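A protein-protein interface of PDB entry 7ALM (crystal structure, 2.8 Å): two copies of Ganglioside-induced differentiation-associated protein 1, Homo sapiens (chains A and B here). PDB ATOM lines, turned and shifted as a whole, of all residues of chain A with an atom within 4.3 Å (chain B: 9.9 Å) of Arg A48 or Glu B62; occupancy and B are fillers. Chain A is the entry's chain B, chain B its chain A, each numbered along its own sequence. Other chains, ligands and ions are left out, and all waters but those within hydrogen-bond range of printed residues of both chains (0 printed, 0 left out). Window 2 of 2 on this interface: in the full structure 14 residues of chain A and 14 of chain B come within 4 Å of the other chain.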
ATOM      1  N   TRP A   9      -8.877 -23.296  -4.093  1.00  0.00           N
ATOM      2  CA  TRP A   9      -7.816 -22.953  -5.028  1.00  0.00           C
ATOM      3  C   TRP A   9      -7.720 -21.433  -5.105  1.00  0.00           C
ATOM      4  O   TRP A   9      -8.717 -20.757  -5.385  1.00  0.00           O
ATOM      5  CB  TRP A   9      -8.074 -23.543  -6.413  1.00  0.00           C
ATOM      6  CG  TRP A   9      -8.314 -25.023  -6.404  1.00  0.00           C
ATOM      7  CD1 TRP A   9      -7.372 -26.010  -6.370  1.00  0.00           C
ATOM      8  CD2 TRP A   9      -9.584 -25.683  -6.434  1.00  0.00           C
ATOM      9  NE1 TRP A   9      -7.978 -27.243  -6.375  1.00  0.00           N
ATOM     10  CE2 TRP A   9      -9.337 -27.069  -6.415  1.00  0.00           C
ATOM     11  CE3 TRP A   9     -10.906 -25.233  -6.474  1.00  0.00           C
ATOM     12  CZ2 TRP A   9     -10.363 -28.009  -6.435  1.00  0.00           C
ATOM     13  CZ3 TRP A   9     -11.919 -26.163  -6.493  1.00  0.00           C
ATOM     14  CH2 TRP A   9     -11.644 -27.537  -6.474  1.00  0.00           C
ATOM     15  N   VAL A  34      -5.031 -25.499  -1.542  1.00  0.00           N
ATOM     16  CA  VAL A  34      -4.621 -26.859  -1.883  1.00  0.00           C
ATOM     17  C   VAL A  34      -3.971 -26.953  -3.252  1.00  0.00           C
ATOM     18  O   VAL A  34      -3.442 -28.016  -3.602  1.00  0.00           O
ATOM     19  CB  VAL A  34      -5.824 -27.821  -1.826  1.00  0.00           C
ATOM     20  CG1 VAL A  34      -6.400 -27.861  -0.422  1.00  0.00           C
ATOM     21  CG2 VAL A  34      -6.892 -27.411  -2.832  1.00  0.00           C
ATOM     22  N   SER A  35      -3.995 -25.880  -4.035  1.00  0.00           N
ATOM     23  CA  SER A  35      -3.365 -25.893  -5.346  1.00  0.00           C
ATOM     24  C   SER A  35      -1.847 -25.852  -5.214  1.00  0.00           C
ATOM     25  O   SER A  35      -1.296 -25.281  -4.268  1.00  0.00           O
ATOM     26  CB  SER A  35      -3.846 -24.705  -6.180  1.00  0.00           C
ATOM     27  OG  SER A  35      -3.494 -23.476  -5.568  1.00  0.00           O
ATOM     28  N   LEU A  36      -1.172 -26.465  -6.175  1.00  0.00           N
ATOM     29  CA  LEU A  36       0.280 -26.476  -6.237  1.00  0.00           C
ATOM     30  C   LEU A  36       0.779 -25.567  -7.353  1.00  0.00           C
ATOM     31  O   LEU A  36       0.064 -25.309  -8.327  1.00  0.00           O
ATOM     32  CB  LEU A  36       0.803 -27.898  -6.470  1.00  0.00           C
ATOM     33  CG  LEU A  36       0.727 -28.843  -5.271  1.00  0.00           C
ATOM     34  CD1 LEU A  36       0.987 -30.273  -5.716  1.00  0.00           C
ATOM     35  CD2 LEU A  36       1.715 -28.423  -4.192  1.00  0.00           C
ATOM     36  N   SER A  39       2.009 -28.543 -11.863  1.00  0.00           N
ATOM     37  CA  SER A  39       1.259 -29.785 -11.918  1.00  0.00           C
ATOM     38  C   SER A  39       2.189 -30.951 -12.247  1.00  0.00           C
ATOM     39  O   SER A  39       3.375 -30.777 -12.536  1.00  0.00           O
ATOM     40  CB  SER A  39       0.143 -29.690 -12.958  1.00  0.00           C
ATOM     41  OG  SER A  39       0.673 -29.521 -14.262  1.00  0.00           O
ATOM     42  N   PRO A  44       1.815 -24.266 -15.095  1.00  0.00           N
ATOM     43  CA  PRO A  44       1.538 -23.286 -14.026  1.00  0.00           C
ATOM     44  C   PRO A  44       0.022 -23.098 -13.850  1.00  0.00           C
ATOM     45  O   PRO A  44      -0.781 -23.649 -14.576  1.00  0.00           O
ATOM     46  CB  PRO A  44       2.217 -22.012 -14.522  1.00  0.00           C
ATOM     47  CG  PRO A  44       2.188 -22.124 -16.008  1.00  0.00           C
ATOM     48  CD  PRO A  44       2.316 -23.597 -16.325  1.00  0.00           C
ATOM     49  N   TRP A  45      -0.344 -22.279 -12.850  1.00  0.00           N
ATOM     50  CA  TRP A  45      -1.764 -22.178 -12.492  1.00  0.00           C
ATOM     51  C   TRP A  45      -2.603 -21.569 -13.612  1.00  0.00           C
ATOM     52  O   TRP A  45      -3.811 -21.834 -13.692  1.00  0.00           O
ATOM     53  CB  TRP A  45      -1.942 -21.366 -11.207  1.00  0.00           C
ATOM     54  CG  TRP A  45      -1.527 -19.927 -11.317  1.00  0.00           C
ATOM     55  CD1 TRP A  45      -0.330 -19.385 -10.944  1.00  0.00           C
ATOM     56  CD2 TRP A  45      -2.314 -18.846 -11.828  1.00  0.00           C
ATOM     57  NE1 TRP A  45      -0.322 -18.034 -11.195  1.00  0.00           N
ATOM     58  CE2 TRP A  45      -1.529 -17.679 -11.737  1.00  0.00           C
ATOM     59  CE3 TRP A  45      -3.605 -18.752 -12.356  1.00  0.00           C
ATOM     60  CZ2 TRP A  45      -1.995 -16.432 -12.153  1.00  0.00           C
ATOM     61  CZ3 TRP A  45      -4.064 -17.516 -12.769  1.00  0.00           C
ATOM     62  CH2 TRP A  45      -3.262 -16.372 -12.665  1.00  0.00           C
ATOM     63  N   PHE A  46      -2.005 -20.755 -14.479  1.00  0.00           N
ATOM     64  CA  PHE A  46      -2.775 -20.125 -15.543  1.00  0.00           C
ATOM     65  C   PHE A  46      -2.986 -21.039 -16.745  1.00  0.00           C
ATOM     66  O   PHE A  46      -3.550 -20.593 -17.749  1.00  0.00           O
ATOM     67  CB  PHE A  46      -2.121 -18.807 -15.986  1.00  0.00           C
ATOM     68  CG  PHE A  46      -0.656 -18.911 -16.302  1.00  0.00           C
ATOM     69  CD1 PHE A  46      -0.227 -19.235 -17.578  1.00  0.00           C
ATOM     70  CD2 PHE A  46       0.293 -18.654 -15.326  1.00  0.00           C
ATOM     71  CE1 PHE A  46       1.125 -19.317 -17.872  1.00  0.00           C
ATOM     72  CE2 PHE A  46       1.645 -18.736 -15.612  1.00  0.00           C
ATOM     73  CZ  PHE A  46       2.061 -19.065 -16.888  1.00  0.00           C
ATOM     74  N   MET A  47      -2.553 -22.298 -16.664  1.00  0.00           N
ATOM     75  CA  MET A  47      -2.916 -23.295 -17.661  1.00  0.00           C
ATOM     76  C   MET A  47      -4.136 -24.103 -17.250  1.00  0.00           C
ATOM     77  O   MET A  47      -4.886 -24.571 -18.112  1.00  0.00           O
ATOM     78  CB  MET A  47      -1.758 -24.265 -17.902  1.00  0.00           C
ATOM     79  CG  MET A  47      -0.592 -23.680 -18.658  1.00  0.00           C
ATOM     80  SD  MET A  47      -1.023 -23.259 -20.353  1.00  0.00           S
ATOM     81  CE  MET A  47       0.545 -22.623 -20.925  1.00  0.00           C
ATOM     82  N   ARG A  48      -4.339 -24.276 -15.950  1.00  0.00           N
ATOM     83  CA  ARG A  48      -5.373 -25.160 -15.431  1.00  0.00           C
ATOM     84  C   ARG A  48      -6.541 -24.346 -14.901  1.00  0.00           C
ATOM     85  O   ARG A  48      -6.916 -24.474 -13.735  1.00  0.00           O
ATOM     86  CB  ARG A  48      -4.780 -26.065 -14.350  1.00  0.00           C
ATOM     87  CG  ARG A  48      -3.670 -26.960 -14.891  1.00  0.00           C
ATOM     88  CD  ARG A  48      -2.753 -27.512 -13.812  1.00  0.00           C
ATOM     89  NE  ARG A  48      -3.465 -28.304 -12.815  1.00  0.00           N
ATOM     90  CZ  ARG A  48      -3.288 -28.196 -11.500  1.00  0.00           C
ATOM     91  NH1 ARG A  48      -2.409 -27.334 -11.003  1.00  0.00           N
ATOM     92  NH2 ARG A  48      -3.984 -28.971 -10.679  1.00  0.00           N
ATOM     93  N   LEU A  49      -7.114 -23.493 -15.755  1.00  0.00           N
ATOM     94  CA  LEU A  49      -8.273 -22.680 -15.418  1.00  0.00           C
ATOM     95  C   LEU A  49      -9.582 -23.434 -15.583  1.00  0.00           C
ATOM     96  O   LEU A  49     -10.646 -22.805 -15.615  1.00  0.00           O
ATOM     97  CB  LEU A  49      -8.289 -21.410 -16.272  1.00  0.00           C
ATOM     98  CG  LEU A  49      -7.011 -20.564 -16.240  1.00  0.00           C
ATOM     99  CD1 LEU A  49      -7.102 -19.354 -17.164  1.00  0.00           C
ATOM    100  CD2 LEU A  49      -6.704 -20.119 -14.816  1.00  0.00           C
ATOM    101  N   ASN A  50      -9.522 -24.758 -15.695  1.00  0.00           N
ATOM    102  CA  ASN A  50     -10.704 -25.587 -15.904  1.00  0.00           C
ATOM    103  C   ASN A  50     -11.849 -25.196 -14.974  1.00  0.00           C
ATOM    104  O   ASN A  50     -13.008 -25.156 -15.387  1.00  0.00           O
ATOM    105  CB  ASN A  50     -10.353 -27.061 -15.698  1.00  0.00           C
ATOM    106  CG  ASN A  50      -9.936 -27.365 -14.274  1.00  0.00           C
ATOM    107  OD1 ASN A  50     -10.779 -27.512 -13.389  1.00  0.00           O
ATOM    108  ND2 ASN A  50      -8.631 -27.463 -14.044  1.00  0.00           N
ATOM    109  N   VAL B   2       0.855 -37.863  -0.182  1.00  0.00           N
ATOM    110  CA  VAL B   2      -0.217 -36.880  -0.307  1.00  0.00           C
ATOM    111  C   VAL B   2      -1.328 -37.284   0.658  1.00  0.00           C
ATOM    112  O   VAL B   2      -1.954 -38.334   0.492  1.00  0.00           O
ATOM    113  CB  VAL B   2      -0.732 -36.787  -1.747  1.00  0.00           C
ATOM    114  CG1 VAL B   2      -1.766 -35.677  -1.876  1.00  0.00           C
ATOM    115  CG2 VAL B   2       0.424 -36.562  -2.713  1.00  0.00           C
ATOM    116  N   LYS B   3      -1.571 -36.454   1.670  1.00  0.00           N
ATOM    117  CA  LYS B   3      -2.511 -36.814   2.722  1.00  0.00           C
ATOM    118  C   LYS B   3      -3.929 -36.937   2.180  1.00  0.00           C
ATOM    119  O   LYS B   3      -4.344 -36.190   1.289  1.00  0.00           O
ATOM    120  CB  LYS B   3      -2.475 -35.771   3.842  1.00  0.00           C
ATOM    121  CG  LYS B   3      -1.240 -35.845   4.726  1.00  0.00           C
ATOM    122  CD  LYS B   3      -1.135 -34.642   5.661  1.00  0.00           C
ATOM    123  CE  LYS B   3      -2.394 -34.457   6.504  1.00  0.00           C
ATOM    124  NZ  LYS B   3      -2.793 -35.711   7.203  1.00  0.00           N
ATOM    125  N   LEU B   4      -4.669 -37.897   2.725  1.00  0.00           N
ATOM    126  CA  LEU B   4      -6.103 -38.021   2.505  1.00  0.00           C
ATOM    127  C   LEU B   4      -6.816 -37.431   3.716  1.00  0.00           C
ATOM    128  O   LEU B   4      -6.583 -37.870   4.848  1.00  0.00           O
ATOM    129  CB  LEU B   4      -6.508 -39.480   2.311  1.00  0.00           C
ATOM    130  CG  LEU B   4      -6.589 -40.017   0.886  1.00  0.00           C
ATOM    131  CD1 LEU B   4      -6.673 -41.535   0.922  1.00  0.00           C
ATOM    132  CD2 LEU B   4      -7.779 -39.437   0.154  1.00  0.00           C
ATOM    133  N   ILE B   5      -7.676 -36.445   3.482  1.00  0.00           N
ATOM    134  CA  ILE B   5      -8.422 -35.783   4.544  1.00  0.00           C
ATOM    135  C   ILE B   5      -9.908 -35.943   4.254  1.00  0.00           C
ATOM    136  O   ILE B   5     -10.352 -35.718   3.123  1.00  0.00           O
ATOM    137  CB  ILE B   5      -8.051 -34.294   4.666  1.00  0.00           C
ATOM    138  CG1 ILE B   5      -6.536 -34.133   4.801  1.00  0.00           C
ATOM    139  CG2 ILE B   5      -8.761 -33.680   5.863  1.00  0.00           C
ATOM    140  CD1 ILE B   5      -6.064 -32.692   4.796  1.00  0.00           C
ATOM    141  N   LEU B  58     -13.937 -34.766   0.767  1.00  0.00           N
ATOM    142  CA  LEU B  58     -12.593 -35.330   0.770  1.00  0.00           C
ATOM    143  C   LEU B  58     -11.622 -34.337   0.149  1.00  0.00           C
ATOM    144  O   LEU B  58     -11.910 -33.761  -0.909  1.00  0.00           O
ATOM    145  CB  LEU B  58     -12.538 -36.650  -0.003  1.00  0.00           C
ATOM    146  CG  LEU B  58     -11.169 -37.340  -0.050  1.00  0.00           C
ATOM    147  CD1 LEU B  58     -10.948 -38.169   1.208  1.00  0.00           C
ATOM    148  CD2 LEU B  58     -11.023 -38.201  -1.297  1.00  0.00           C
ATOM    149  N   ILE B  59     -10.474 -34.155   0.793  1.00  0.00           N
ATOM    150  CA  ILE B  59      -9.371 -33.372   0.250  1.00  0.00           C
ATOM    151  C   ILE B  59      -8.193 -34.318   0.051  1.00  0.00           C
ATOM    152  O   ILE B  59      -7.721 -34.937   1.014  1.00  0.00           O
ATOM    153  CB  ILE B  59      -8.981 -32.203   1.168  1.00  0.00           C
ATOM    154  CG1 ILE B  59     -10.156 -31.239   1.348  1.00  0.00           C
ATOM    155  CG2 ILE B  59      -7.768 -31.466   0.604  1.00  0.00           C
ATOM    156  CD1 ILE B  59     -10.872 -31.386   2.675  1.00  0.00           C
ATOM    157  N   HIS B  60      -7.724 -34.435  -1.185  1.00  0.00           N
ATOM    158  CA  HIS B  60      -6.585 -35.283  -1.516  1.00  0.00           C
ATOM    159  C   HIS B  60      -5.670 -34.471  -2.422  1.00  0.00           C
ATOM    160  O   HIS B  60      -5.876 -34.411  -3.641  1.00  0.00           O
ATOM    161  CB  HIS B  60      -7.028 -36.588  -2.172  1.00  0.00           C
ATOM    162  CG  HIS B  60      -5.896 -37.517  -2.478  1.00  0.00           C
ATOM    163  ND1 HIS B  60      -5.775 -38.163  -3.687  1.00  0.00           N
ATOM    164  CD2 HIS B  60      -4.827 -37.894  -1.739  1.00  0.00           C
ATOM    165  CE1 HIS B  60      -4.683 -38.907  -3.678  1.00  0.00           C
ATOM    166  NE2 HIS B  60      -4.089 -38.760  -2.508  1.00  0.00           N
ATOM    167  N   GLY B  61      -4.674 -33.836  -1.826  1.00  0.00           N
ATOM    168  CA  GLY B  61      -3.791 -32.974  -2.592  1.00  0.00           C
ATOM    169  C   GLY B  61      -4.557 -31.804  -3.174  1.00  0.00           C
ATOM    170  O   GLY B  61      -5.173 -31.010  -2.453  1.00  0.00           O
ATOM    171  N   GLU B  62      -4.527 -31.685  -4.499  1.00  0.00           N
ATOM    172  CA  GLU B  62      -5.175 -30.574  -5.184  1.00  0.00           C
ATOM    173  C   GLU B  62      -6.665 -30.792  -5.422  1.00  0.00           C
ATOM    174  O   GLU B  62      -7.321 -29.897  -5.964  1.00  0.00           O
ATOM    175  CB  GLU B  62      -4.488 -30.317  -6.529  1.00  0.00           C
ATOM    176  CG  GLU B  62      -3.096 -29.728  -6.421  1.00  0.00           C
ATOM    177  CD  GLU B  62      -2.508 -29.389  -7.777  1.00  0.00           C
ATOM    178  OE1 GLU B  62      -2.588 -30.243  -8.684  1.00  0.00           O
ATOM    179  OE2 GLU B  62      -1.982 -28.267  -7.942  1.00  0.00           O
ATOM    180  N   ASN B  63      -7.219 -31.936  -5.033  1.00  0.00           N
ATOM    181  CA  ASN B  63      -8.595 -32.285  -5.358  1.00  0.00           C
ATOM    182  C   ASN B  63      -9.493 -32.156  -4.137  1.00  0.00           C
ATOM    183  O   ASN B  63      -9.127 -32.572  -3.032  1.00  0.00           O
ATOM    184  CB  ASN B  63      -8.678 -33.709  -5.913  1.00  0.00           C
ATOM    185  CG  ASN B  63      -8.065 -33.830  -7.289  1.00  0.00           C
ATOM    186  OD1 ASN B  63      -7.128 -34.600  -7.500  1.00  0.00           O
ATOM    187  ND2 ASN B  63      -8.589 -33.064  -8.238  1.00  0.00           N
ATOM    188  N   ILE B  64     -10.670 -31.570  -4.349  1.00  0.00           N
ATOM    189  CA  ILE B  64     -11.706 -31.435  -3.332  1.00  0.00           C
ATOM    190  C   ILE B  64     -12.982 -32.031  -3.909  1.00  0.00           C
ATOM    191  O   ILE B  64     -13.498 -31.537  -4.920  1.00  0.00           O
ATOM    192  CB  ILE B  64     -11.931 -29.969  -2.927  1.00  0.00           C
ATOM    193  CG1 ILE B  64     -10.677 -29.397  -2.263  1.00  0.00           C
ATOM    194  CG2 ILE B  64     -13.126 -29.859  -1.995  1.00  0.00           C
ATOM    195  CD1 ILE B  64     -10.634 -27.882  -2.233  1.00  0.00           C
ATOM    196  N   ILE B  65     -13.489 -33.086  -3.280  1.00  0.00           N
ATOM    197  CA  ILE B  65     -14.645 -33.816  -3.786  1.00  0.00           C
ATOM    198  C   ILE B  65     -15.707 -33.859  -2.694  1.00  0.00           C
ATOM    199  O   ILE B  65     -15.436 -34.309  -1.572  1.00  0.00           O
ATOM    200  CB  ILE B  65     -14.270 -35.236  -4.238  1.00  0.00           C
ATOM    201  CG1 ILE B  65     -13.052 -35.213  -5.167  1.00  0.00           C
ATOM    202  CG2 ILE B  65     -15.439 -35.892  -4.954  1.00  0.00           C
ATOM    203  CD1 ILE B  65     -11.725 -35.332  -4.446  1.00  0.00           C
ATOM    204  N   TYR B  74     -14.093 -41.160  -6.935  1.00  0.00           N
ATOM    205  CA  TYR B  74     -12.740 -40.621  -6.949  1.00  0.00           C
ATOM    206  C   TYR B  74     -11.743 -41.614  -6.363  1.00  0.00           C
ATOM    207  O   TYR B  74     -10.640 -41.783  -6.894  1.00  0.00           O
ATOM    208  CB  TYR B  74     -12.691 -39.301  -6.179  1.00  0.00           C
ATOM    209  CG  TYR B  74     -11.311 -38.688  -6.125  1.00  0.00           C
ATOM    210  CD1 TYR B  74     -10.811 -37.970  -7.199  1.00  0.00           C
ATOM    211  CD2 TYR B  74     -10.508 -38.833  -5.002  1.00  0.00           C
ATOM    212  CE1 TYR B  74      -9.551 -37.410  -7.156  1.00  0.00           C
ATOM    213  CE2 TYR B  74      -9.245 -38.278  -4.952  1.00  0.00           C
ATOM    214  CZ  TYR B  74      -8.773 -37.566  -6.030  1.00  0.00           C
ATOM    215  OH  TYR B  74      -7.515 -37.008  -5.987  1.00  0.00           O
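Of the printed residues of chain B, Trp A9 touches Glu B62 (2.8 Å).
Printed residues of chain B within 4 Å of Val A34: Ile B59 (3.99 Å), Gly B61 (3.3 Å), Glu B62 (3.3 Å) and Ile B64 (3.8 Å).
Of the printed residues of chain B, Ser A35 touches Glu B62 (3.6 Å).
Of the printed residues of chain B, Leu A36 touches Glu B62 (2.7 Å).
Of chain B, only Glu B62 comes within 4 Å of Arg A48.
No residue of chain B comes within 4 Å of Leu A49.
Of the printed residues of chain A, Ile B59 touches Val A34.
Printed residues of chain A within 4 Å of Gly B61: Val A34.
Of the printed residues of chain A, Glu B62 touches Trp A9, Val A34, Ser A35, Leu A36 and Arg A48.
Of the printed residues of chain A, Ile B64 touches Val A34 (3.8 Å).
The nearest residue of chain B that does not touch Arg A48 is Asn B63 (6.6 Å).
The nearest printed residue of chain A that does not touch Ile B59 is Trp A9 (8.2 Å).
Ile B59 touches Val A34.
Val A34 touches Gly B61.
Val A34 touches Glu B62.
Val A34 touches Ile B64.
OE2 of Glu B62 touches C of Ser A35 (3.6 Å).
O of Ile B5 lies within hydrogen-bond range of N of Ile B59, at 2.8 Å.
ND2 of Asn A50 sits at hydrogen-bond distance from O of Arg A48 (3.5 Å).
Printed residues of chain B that touch a printed residue of chain A: Ile B59, Gly B61, Glu B62 and Ile B64.
Hydrophobic or aromatic side chains of chain B that line the printed part of chain A: Ile B59 and Ile B64.
Printed residues of chain A that touch a printed residue of chain B: Trp A9, Val A34, Ser A35, Leu A36 and Arg A48.
Among the printed residues, 8 pairs touch across the chains.
The backbone carbonyl oxygen of Glu B62 lies within hydrogen-bond range of the indole nitrogen of Trp A9.
OE2 of Glu B62 is in hydrogen-bond range of N of Leu A36 (2.7 Å).
The side-chain carboxylate (OE1) of Glu B62 lies within salt-bridge range of the guanidinium group (NH2) of Arg A48, 2.7 Å away.
No position is printed for both chains.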
